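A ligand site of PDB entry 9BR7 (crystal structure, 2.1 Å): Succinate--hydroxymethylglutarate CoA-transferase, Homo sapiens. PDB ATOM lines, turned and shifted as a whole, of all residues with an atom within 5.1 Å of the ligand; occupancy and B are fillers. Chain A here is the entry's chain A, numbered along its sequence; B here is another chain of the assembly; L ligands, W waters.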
ATOM      1  N   VAL A  26     -25.431  11.341 -13.063  1.00  0.00           N
ATOM      2  CA  VAL A  26     -24.941  10.768 -11.808  1.00  0.00           C
ATOM      3  C   VAL A  26     -24.781   9.259 -11.928  1.00  0.00           C
ATOM      4  O   VAL A  26     -23.949   8.779 -12.709  1.00  0.00           O
ATOM      5  CB  VAL A  26     -25.854  11.144 -10.618  1.00  0.00           C
ATOM      6  CG1 VAL A  26     -25.161  10.833  -9.305  1.00  0.00           C
ATOM      7  CG2 VAL A  26     -26.217  12.623 -10.693  1.00  0.00           C
ATOM      8  N   LEU A  27     -25.553   8.490 -11.162  1.00  0.00           N
ATOM      9  CA  LEU A  27     -25.291   7.054 -11.065  1.00  0.00           C
ATOM     10  C   LEU A  27     -26.496   6.163 -11.377  1.00  0.00           C
ATOM     11  O   LEU A  27     -26.406   5.283 -12.235  1.00  0.00           O
ATOM     12  CB  LEU A  27     -24.767   6.707  -9.678  1.00  0.00           C
ATOM     13  CG  LEU A  27     -24.577   5.217  -9.412  1.00  0.00           C
ATOM     14  CD1 LEU A  27     -23.588   4.611 -10.389  1.00  0.00           C
ATOM     15  CD2 LEU A  27     -24.115   4.988  -7.981  1.00  0.00           C
ATOM     16  N   THR A  55     -20.920  13.922 -13.119  1.00  0.00           N
ATOM     17  CA  THR A  55     -19.768  13.107 -12.739  1.00  0.00           C
ATOM     18  C   THR A  55     -18.492  13.542 -13.457  1.00  0.00           C
ATOM     19  O   THR A  55     -17.393  13.213 -13.003  1.00  0.00           O
ATOM     20  CB  THR A  55     -20.041  11.637 -13.012  1.00  0.00           C
ATOM     21  OG1 THR A  55     -20.263  11.438 -14.412  1.00  0.00           O
ATOM     22  CG2 THR A  55     -21.266  11.165 -12.251  1.00  0.00           C
ATOM     23  N   TRP A  58     -16.333  15.613 -11.053  1.00  0.00           N
ATOM     24  CA  TRP A  58     -16.066  15.077  -9.719  1.00  0.00           C
ATOM     25  C   TRP A  58     -14.715  14.375  -9.735  1.00  0.00           C
ATOM     26  O   TRP A  58     -14.603  13.181 -10.055  1.00  0.00           O
ATOM     27  CB  TRP A  58     -17.189  14.148  -9.296  1.00  0.00           C
ATOM     28  CG  TRP A  58     -18.465  14.887  -9.053  1.00  0.00           C
ATOM     29  CD1 TRP A  58     -18.613  16.246  -8.970  1.00  0.00           C
ATOM     30  CD2 TRP A  58     -19.784  14.332  -8.915  1.00  0.00           C
ATOM     31  NE1 TRP A  58     -19.936  16.569  -8.762  1.00  0.00           N
ATOM     32  CE2 TRP A  58     -20.671  15.410  -8.725  1.00  0.00           C
ATOM     33  CE3 TRP A  58     -20.291  13.028  -8.933  1.00  0.00           C
ATOM     34  CZ2 TRP A  58     -22.043  15.223  -8.551  1.00  0.00           C
ATOM     35  CZ3 TRP A  58     -21.649  12.850  -8.756  1.00  0.00           C
ATOM     36  CH2 TRP A  58     -22.512  13.944  -8.570  1.00  0.00           C
ATOM     37  N   TYR A  69     -15.136   8.753 -11.782  1.00  0.00           N
ATOM     38  CA  TYR A  69     -16.568   8.651 -11.534  1.00  0.00           C
ATOM     39  C   TYR A  69     -17.324   8.473 -12.848  1.00  0.00           C
ATOM     40  O   TYR A  69     -18.100   7.533 -13.014  1.00  0.00           O
ATOM     41  CB  TYR A  69     -17.072   9.901 -10.806  1.00  0.00           C
ATOM     42  CG  TYR A  69     -17.124   9.783  -9.297  1.00  0.00           C
ATOM     43  CD1 TYR A  69     -18.088   9.006  -8.679  1.00  0.00           C
ATOM     44  CD2 TYR A  69     -16.210  10.464  -8.501  1.00  0.00           C
ATOM     45  CE1 TYR A  69     -18.140   8.902  -7.296  1.00  0.00           C
ATOM     46  CE2 TYR A  69     -16.260  10.379  -7.124  1.00  0.00           C
ATOM     47  CZ  TYR A  69     -17.223   9.595  -6.528  1.00  0.00           C
ATOM     48  OH  TYR A  69     -17.274   9.500  -5.148  1.00  0.00           O
ATOM     49  N   SER A  72     -16.570   5.185 -14.885  1.00  0.00           N
ATOM     50  CA  SER A  72     -16.935   3.896 -14.309  1.00  0.00           C
ATOM     51  C   SER A  72     -18.297   3.408 -14.795  1.00  0.00           C
ATOM     52  O   SER A  72     -18.540   2.200 -14.820  1.00  0.00           O
ATOM     53  CB  SER A  72     -16.916   3.974 -12.778  1.00  0.00           C
ATOM     54  OG  SER A  72     -17.907   4.862 -12.294  1.00  0.00           O
ATOM     55  N   VAL A  73     -19.208   4.312 -15.181  1.00  0.00           N
ATOM     56  CA  VAL A  73     -20.573   3.890 -15.491  1.00  0.00           C
ATOM     57  C   VAL A  73     -21.100   4.525 -16.767  1.00  0.00           C
ATOM     58  O   VAL A  73     -22.302   4.782 -16.889  1.00  0.00           O
ATOM     59  CB  VAL A  73     -21.515   4.214 -14.310  1.00  0.00           C
ATOM     60  CG1 VAL A  73     -21.107   3.427 -13.067  1.00  0.00           C
ATOM     61  CG2 VAL A  73     -21.532   5.707 -14.036  1.00  0.00           C
ATOM     62  N   GLY A 148     -33.591  13.164  -5.389  1.00  0.00           N
ATOM     63  CA  GLY A 148     -33.186  11.861  -4.894  1.00  0.00           C
ATOM     64  C   GLY A 148     -31.694  11.795  -4.634  1.00  0.00           C
ATOM     65  O   GLY A 148     -30.884  12.237  -5.450  1.00  0.00           O
ATOM     66  N   TYR A 149     -31.331  11.253  -3.476  1.00  0.00           N
ATOM     67  CA  TYR A 149     -29.940  11.023  -3.108  1.00  0.00           C
ATOM     68  C   TYR A 149     -29.835   9.678  -2.414  1.00  0.00           C
ATOM     69  O   TYR A 149     -30.684   9.328  -1.592  1.00  0.00           O
ATOM     70  CB  TYR A 149     -29.406  12.135  -2.192  1.00  0.00           C
ATOM     71  CG  TYR A 149     -29.512  13.525  -2.774  1.00  0.00           C
ATOM     72  CD1 TYR A 149     -28.517  14.036  -3.587  1.00  0.00           C
ATOM     73  CD2 TYR A 149     -30.621  14.322  -2.507  1.00  0.00           C
ATOM     74  CE1 TYR A 149     -28.605  15.309  -4.127  1.00  0.00           C
ATOM     75  CE2 TYR A 149     -30.718  15.597  -3.043  1.00  0.00           C
ATOM     76  CZ  TYR A 149     -29.714  16.079  -3.842  1.00  0.00           C
ATOM     77  OH  TYR A 149     -29.812  17.346  -4.375  1.00  0.00           O
ATOM     78  N   ASP A 150     -28.790   8.919  -2.762  1.00  0.00           N
ATOM     79  CA  ASP A 150     -28.663   7.570  -2.211  1.00  0.00           C
ATOM     80  C   ASP A 150     -28.590   7.608  -0.683  1.00  0.00           C
ATOM     81  O   ASP A 150     -29.310   6.867  -0.003  1.00  0.00           O
ATOM     82  CB  ASP A 150     -27.427   6.879  -2.795  1.00  0.00           C
ATOM     83  CG  ASP A 150     -27.181   5.510  -2.180  1.00  0.00           C
ATOM     84  OD1 ASP A 150     -26.842   5.439  -0.979  1.00  0.00           O
ATOM     85  OD2 ASP A 150     -27.347   4.491  -2.890  1.00  0.00           O
ATOM     86  N   ALA A 151     -27.732   8.466  -0.129  1.00  0.00           N
ATOM     87  CA  ALA A 151     -27.578   8.509   1.317  1.00  0.00           C
ATOM     88  C   ALA A 151     -28.874   8.930   1.993  1.00  0.00           C
ATOM     89  O   ALA A 151     -29.232   8.415   3.062  1.00  0.00           O
ATOM     90  CB  ALA A 151     -26.434   9.441   1.702  1.00  0.00           C
ATOM     91  N   GLY A 174     -20.710   0.948   1.553  1.00  0.00           N
ATOM     92  CA  GLY A 174     -19.542   1.561   0.951  1.00  0.00           C
ATOM     93  C   GLY A 174     -19.824   2.180  -0.397  1.00  0.00           C
ATOM     94  O   GLY A 174     -19.226   3.198  -0.753  1.00  0.00           O
ATOM     95  N   VAL A 175     -20.735   1.584  -1.158  1.00  0.00           N
ATOM     96  CA  VAL A 175     -21.186   2.133  -2.436  1.00  0.00           C
ATOM     97  C   VAL A 175     -22.677   2.404  -2.343  1.00  0.00           C
ATOM     98  O   VAL A 175     -23.374   1.905  -1.452  1.00  0.00           O
ATOM     99  CB  VAL A 175     -20.872   1.184  -3.613  1.00  0.00           C
ATOM    100  CG1 VAL A 175     -19.368   1.061  -3.804  1.00  0.00           C
ATOM    101  CG2 VAL A 175     -21.496  -0.182  -3.373  1.00  0.00           C
ATOM    102  N   ALA A 176     -23.164   3.210  -3.286  1.00  0.00           N
ATOM    103  CA  ALA A 176     -24.561   3.656  -3.300  1.00  0.00           C
ATOM    104  C   ALA A 176     -25.450   2.505  -3.790  1.00  0.00           C
ATOM    105  O   ALA A 176     -25.973   2.504  -4.903  1.00  0.00           O
ATOM    106  CB  ALA A 176     -24.723   4.895  -4.156  1.00  0.00           C
ATOM    107  N   ASP A 179     -28.942   3.466  -5.060  1.00  0.00           N
ATOM    108  CA  ASP A 179     -28.913   3.933  -6.441  1.00  0.00           C
ATOM    109  C   ASP A 179     -28.754   2.757  -7.404  1.00  0.00           C
ATOM    110  O   ASP A 179     -29.471   2.659  -8.407  1.00  0.00           O
ATOM    111  CB  ASP A 179     -27.768   4.934  -6.622  1.00  0.00           C
ATOM    112  CG  ASP A 179     -28.173   6.360  -6.306  1.00  0.00           C
ATOM    113  OD1 ASP A 179     -29.376   6.609  -6.077  1.00  0.00           O
ATOM    114  OD2 ASP A 179     -27.284   7.228  -6.285  1.00  0.00           O
ATOM    115  N   LEU B 218     -19.068  -2.062  -7.238  1.00  0.00           N
ATOM    116  CA  LEU B 218     -17.984  -1.215  -6.749  1.00  0.00           C
ATOM    117  C   LEU B 218     -17.736  -0.036  -7.672  1.00  0.00           C
ATOM    118  O   LEU B 218     -17.368   1.048  -7.202  1.00  0.00           O
ATOM    119  CB  LEU B 218     -16.711  -2.051  -6.586  1.00  0.00           C
ATOM    120  CG  LEU B 218     -16.758  -3.124  -5.497  1.00  0.00           C
ATOM    121  CD1 LEU B 218     -15.411  -3.819  -5.356  1.00  0.00           C
ATOM    122  CD2 LEU B 218     -17.222  -2.549  -4.163  1.00  0.00           C
ATOM    123  N   SER B 219     -17.938  -0.218  -8.974  1.00  0.00           N
ATOM    124  CA  SER B 219     -17.881   0.849  -9.975  1.00  0.00           C
ATOM    125  C   SER B 219     -16.686   1.772  -9.767  1.00  0.00           C
ATOM    126  O   SER B 219     -15.533   1.363  -9.957  1.00  0.00           O
ATOM    127  CB  SER B 219     -19.184   1.650  -9.960  1.00  0.00           C
ATOM    128  OG  SER B 219     -19.374   2.322  -8.727  1.00  0.00           O
ATOM    129  N   HIS B 220     -16.943   3.031  -9.409  1.00  0.00           N
ATOM    130  CA  HIS B 220     -15.872   4.024  -9.375  1.00  0.00           C
ATOM    131  C   HIS B 220     -14.811   3.669  -8.338  1.00  0.00           C
ATOM    132  O   HIS B 220     -13.616   3.937  -8.542  1.00  0.00           O
ATOM    133  CB  HIS B 220     -16.442   5.423  -9.125  1.00  0.00           C
ATOM    134  CG  HIS B 220     -16.615   5.759  -7.672  1.00  0.00           C
ATOM    135  ND1 HIS B 220     -17.724   5.365  -6.948  1.00  0.00           N
ATOM    136  CD2 HIS B 220     -15.848   6.469  -6.818  1.00  0.00           C
ATOM    137  CE1 HIS B 220     -17.621   5.805  -5.711  1.00  0.00           C
ATOM    138  NE2 HIS B 220     -16.487   6.474  -5.604  1.00  0.00           N
ATOM    139  N   ILE B 242     -16.822  15.184  -0.831  1.00  0.00           N
ATOM    140  CA  ILE B 242     -17.839  16.201  -0.592  1.00  0.00           C
ATOM    141  C   ILE B 242     -18.043  16.356   0.908  1.00  0.00           C
ATOM    142  O   ILE B 242     -18.301  15.374   1.609  1.00  0.00           O
ATOM    143  CB  ILE B 242     -19.179  15.847  -1.288  1.00  0.00           C
ATOM    144  CG1 ILE B 242     -18.990  15.827  -2.803  1.00  0.00           C
ATOM    145  CG2 ILE B 242     -20.254  16.836  -0.893  1.00  0.00           C
ATOM    146  CD1 ILE B 242     -20.169  15.259  -3.564  1.00  0.00           C
ATOM    147  N   TYR B 245     -21.466  16.113   4.161  1.00  0.00           N
ATOM    148  CA  TYR B 245     -22.479  15.205   3.610  1.00  0.00           C
ATOM    149  C   TYR B 245     -22.359  13.892   4.380  1.00  0.00           C
ATOM    150  O   TYR B 245     -21.537  13.049   4.028  1.00  0.00           O
ATOM    151  CB  TYR B 245     -22.288  14.991   2.119  1.00  0.00           C
ATOM    152  CG  TYR B 245     -23.411  14.202   1.488  1.00  0.00           C
ATOM    153  CD1 TYR B 245     -24.661  14.150   2.091  1.00  0.00           C
ATOM    154  CD2 TYR B 245     -23.221  13.492   0.309  1.00  0.00           C
ATOM    155  CE1 TYR B 245     -25.697  13.422   1.529  1.00  0.00           C
ATOM    156  CE2 TYR B 245     -24.246  12.771  -0.260  1.00  0.00           C
ATOM    157  CZ  TYR B 245     -25.487  12.733   0.358  1.00  0.00           C
ATOM    158  OH  TYR B 245     -26.513  12.012  -0.210  1.00  0.00           O
ATOM    159  N   ALA B 259     -24.464  19.321   1.577  1.00  0.00           N
ATOM    160  CA  ALA B 259     -24.364  20.549   0.809  1.00  0.00           C
ATOM    161  C   ALA B 259     -23.528  20.243  -0.431  1.00  0.00           C
ATOM    162  O   ALA B 259     -22.328  20.003  -0.324  1.00  0.00           O
ATOM    163  CB  ALA B 259     -23.733  21.679   1.621  1.00  0.00           C
ATOM    164  N   GLY B 260     -24.173  20.242  -1.601  1.00  0.00           N
ATOM    165  CA  GLY B 260     -23.509  19.900  -2.834  1.00  0.00           C
ATOM    166  C   GLY B 260     -22.753  21.017  -3.509  1.00  0.00           C
ATOM    167  O   GLY B 260     -22.092  20.774  -4.529  1.00  0.00           O
ATOM    168  N   GLN B 264     -25.491  25.821  -1.281  1.00  0.00           N
ATOM    169  CA  GLN B 264     -26.157  24.943  -0.334  1.00  0.00           C
ATOM    170  C   GLN B 264     -25.469  24.965   1.025  1.00  0.00           C
ATOM    171  O   GLN B 264     -26.136  24.909   2.064  1.00  0.00           O
ATOM    172  CB  GLN B 264     -26.209  23.520  -0.896  1.00  0.00           C
ATOM    173  CG  GLN B 264     -27.238  23.342  -1.999  1.00  0.00           C
ATOM    174  CD  GLN B 264     -27.306  21.923  -2.521  1.00  0.00           C
ATOM    175  OE1 GLN B 264     -26.504  21.068  -2.132  1.00  0.00           O
ATOM    176  NE2 GLN B 264     -28.269  21.652  -3.383  1.00  0.00           N
ATOM    177  N   PRO B 322     -29.944  18.359   0.248  1.00  0.00           N
ATOM    178  CA  PRO B 322     -30.181  16.944   0.584  1.00  0.00           C
ATOM    179  C   PRO B 322     -30.257  16.777   2.094  1.00  0.00           C
ATOM    180  O   PRO B 322     -29.304  17.091   2.815  1.00  0.00           O
ATOM    181  CB  PRO B 322     -28.955  16.230  -0.012  1.00  0.00           C
ATOM    182  CG  PRO B 322     -27.916  17.294  -0.139  1.00  0.00           C
ATOM    183  CD  PRO B 322     -28.647  18.578  -0.406  1.00  0.00           C
HETATM  184  C1  LIG L   1     -21.259   8.134  -9.567  1.00  0.00           C
HETATM  185  C2  LIG L   1     -21.644   9.989  -7.066  1.00  0.00           C
HETATM  186  C3  LIG L   1     -23.454  10.452  -5.509  1.00  0.00           C
HETATM  187  C4  LIG L   1     -26.876  12.875  -6.458  1.00  0.00           C
HETATM  188  C5  LIG L   1     -23.642  14.263  -5.476  1.00  0.00           C
HETATM  189  C6  LIG L   1     -24.879  14.992  -3.298  1.00  0.00           C
HETATM  190  C7  LIG L   1     -20.866   6.010  -6.502  1.00  0.00           C
HETATM  191  C8  LIG L   1     -20.811   6.520  -7.872  1.00  0.00           C
HETATM  192  C9  LIG L   1     -20.171   5.712  -8.813  1.00  0.00           C
HETATM  193  C10 LIG L   1     -20.066   6.109 -10.145  1.00  0.00           C
HETATM  194  C11 LIG L   1     -20.618   7.336 -10.511  1.00  0.00           C
HETATM  195  C12 LIG L   1     -21.385   7.765  -8.222  1.00  0.00           C
HETATM  196  C13 LIG L   1     -22.090   8.692  -7.304  1.00  0.00           C
HETATM  197  C14 LIG L   1     -22.308  10.853  -6.195  1.00  0.00           C
HETATM  198  C15 LIG L   1     -24.181  11.382  -4.593  1.00  0.00           C
HETATM  199  C16 LIG L   1     -26.354  11.783  -5.775  1.00  0.00           C
HETATM  200  C17 LIG L   1     -26.950  10.409  -5.512  1.00  0.00           C
HETATM  201  C18 LIG L   1     -24.903  13.512  -5.775  1.00  0.00           C
HETATM  202  C19 LIG L   1     -23.594  15.042  -4.128  1.00  0.00           C
HETATM  203  C20 LIG L   1     -25.137  16.272  -2.495  1.00  0.00           C
HETATM  204  C21 LIG L   1     -23.913   9.155  -5.753  1.00  0.00           C
HETATM  205  C22 LIG L   1     -23.244   8.303  -6.617  1.00  0.00           C
HETATM  206  N1  LIG L   1     -20.621   4.669  -6.140  1.00  0.00           N
HETATM  207  N2  LIG L   1     -20.744   4.571  -4.772  1.00  0.00           N
HETATM  208  N3  LIG L   1     -21.043   5.765  -4.335  1.00  0.00           N
HETATM  209  N4  LIG L   1     -21.119   6.671  -5.339  1.00  0.00           N
HETATM  210  N5  LIG L   1     -25.105  12.199  -5.333  1.00  0.00           N
HETATM  211  N6  LIG L   1     -25.981  13.958  -6.458  1.00  0.00           N
HETATM  212  O1  LIG L   1     -26.916  10.007  -4.331  1.00  0.00           O
HETATM  213  O2  LIG L   1     -27.402   9.808  -6.511  1.00  0.00           O
HETATM  214 CL1  LIG L   1     -28.377  12.950  -7.210  1.00  0.00          CL
HETATM  215  O   HOH W   1     -21.311   6.514  -1.796  1.00  0.00           O
HETATM  216  O   HOH W   2     -20.179   9.135  -3.923  1.00  0.00           O
HETATM  217  O   HOH W   3     -26.867  16.366  -7.713  1.00  0.00           O
HETATM  218  O   HOH W   4     -30.972  14.065  -7.480  1.00  0.00           O
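An oxygen (O1) of the ligand lies within hydrogen-bond range of the backbone NH of Asp 150, 2.7 Å away.
N of Ala 176 lies within hydrogen-bond range of N2 of the ligand (3.1 Å).
The side-chain carboxylate (OD2) of Asp 179 lies close to an oxygen (O2) of the ligand.
A ring nitrogen (ND1) of His 220 of chain B is in hydrogen-bond range of a nitrogen (N1) of the ligand (3.1 Å).
N of Asp 179 is in hydrogen-bond range of OD2 of Asp 150, 2.9 Å away.
A ring nitrogen (NE2) of His 220 of chain B sits at hydrogen-bond distance from the side-chain hydroxyl (OH) of Tyr 69 (3.2 Å).
O of Tyr 69 is in hydrogen-bond range of OG of Ser 72 (2.8 Å).
The backbone NH (N) of Gly 260 of chain B lies within hydrogen-bond range of the side-chain amide oxygen (OE1) of Gln 264 of chain B (2.5 Å).
Water W2 lies within hydrogen-bond range of a nitrogen (N4) of the ligand (3.0 Å) and the side-chain hydroxyl (OH) of Tyr 69 (3.2 Å).
CG1 of Val 26 touches O2 of the ligand, 3.7 Å away.
Leu 27 touches the ligand.
Trp 58 touches the ligand.
Tyr 69 touches the ligand.
OG of Ser 72 touches C10 of the ligand, 3.3 Å away.
Val 73 touches the ligand (CG2 to C11, 3.99 Å).
O of Gly 148 touches CL1 of the ligand, at 3.1 Å.
Tyr 149 touches the ligand.
Val 175 touches the ligand (CA to N2, 3.4 Å).
Ser 219 of chain B touches the ligand.
Ile 242 of chain B touches the ligand.
CE2 of Tyr 245 of chain B touches C6 of the ligand (3.8 Å).
CA of Gly 260 of chain B touches C20 of the ligand, 3.99 Å away.
Pro 322 of chain B touches the ligand.
Hydrophobic or aromatic side chains within 4 Å of the ligand: Val 26, Leu 27, Trp 58, Tyr 69, Val 73, Tyr 149, Val 175, Ala 176, His 220 of chain B, Ile 242 of chain B, Tyr 245 of chain B and Pro 322 of chain B.
18 residues have an atom within 4 Å of the ligand: Val 26, Leu 27, Trp 58, Tyr 69, Ser 72, Val 73, Gly 148, Tyr 149, Asp 150, Val 175, Ala 176, Asp 179, Ser 219 of chain B, His 220 of chain B, Ile 242 of chain B, Tyr 245 of chain B, Gly 260 of chain B and Pro 322 of chain B.
The nearest printed residue that does not touch the ligand is Thr 55 (4.05 Å).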
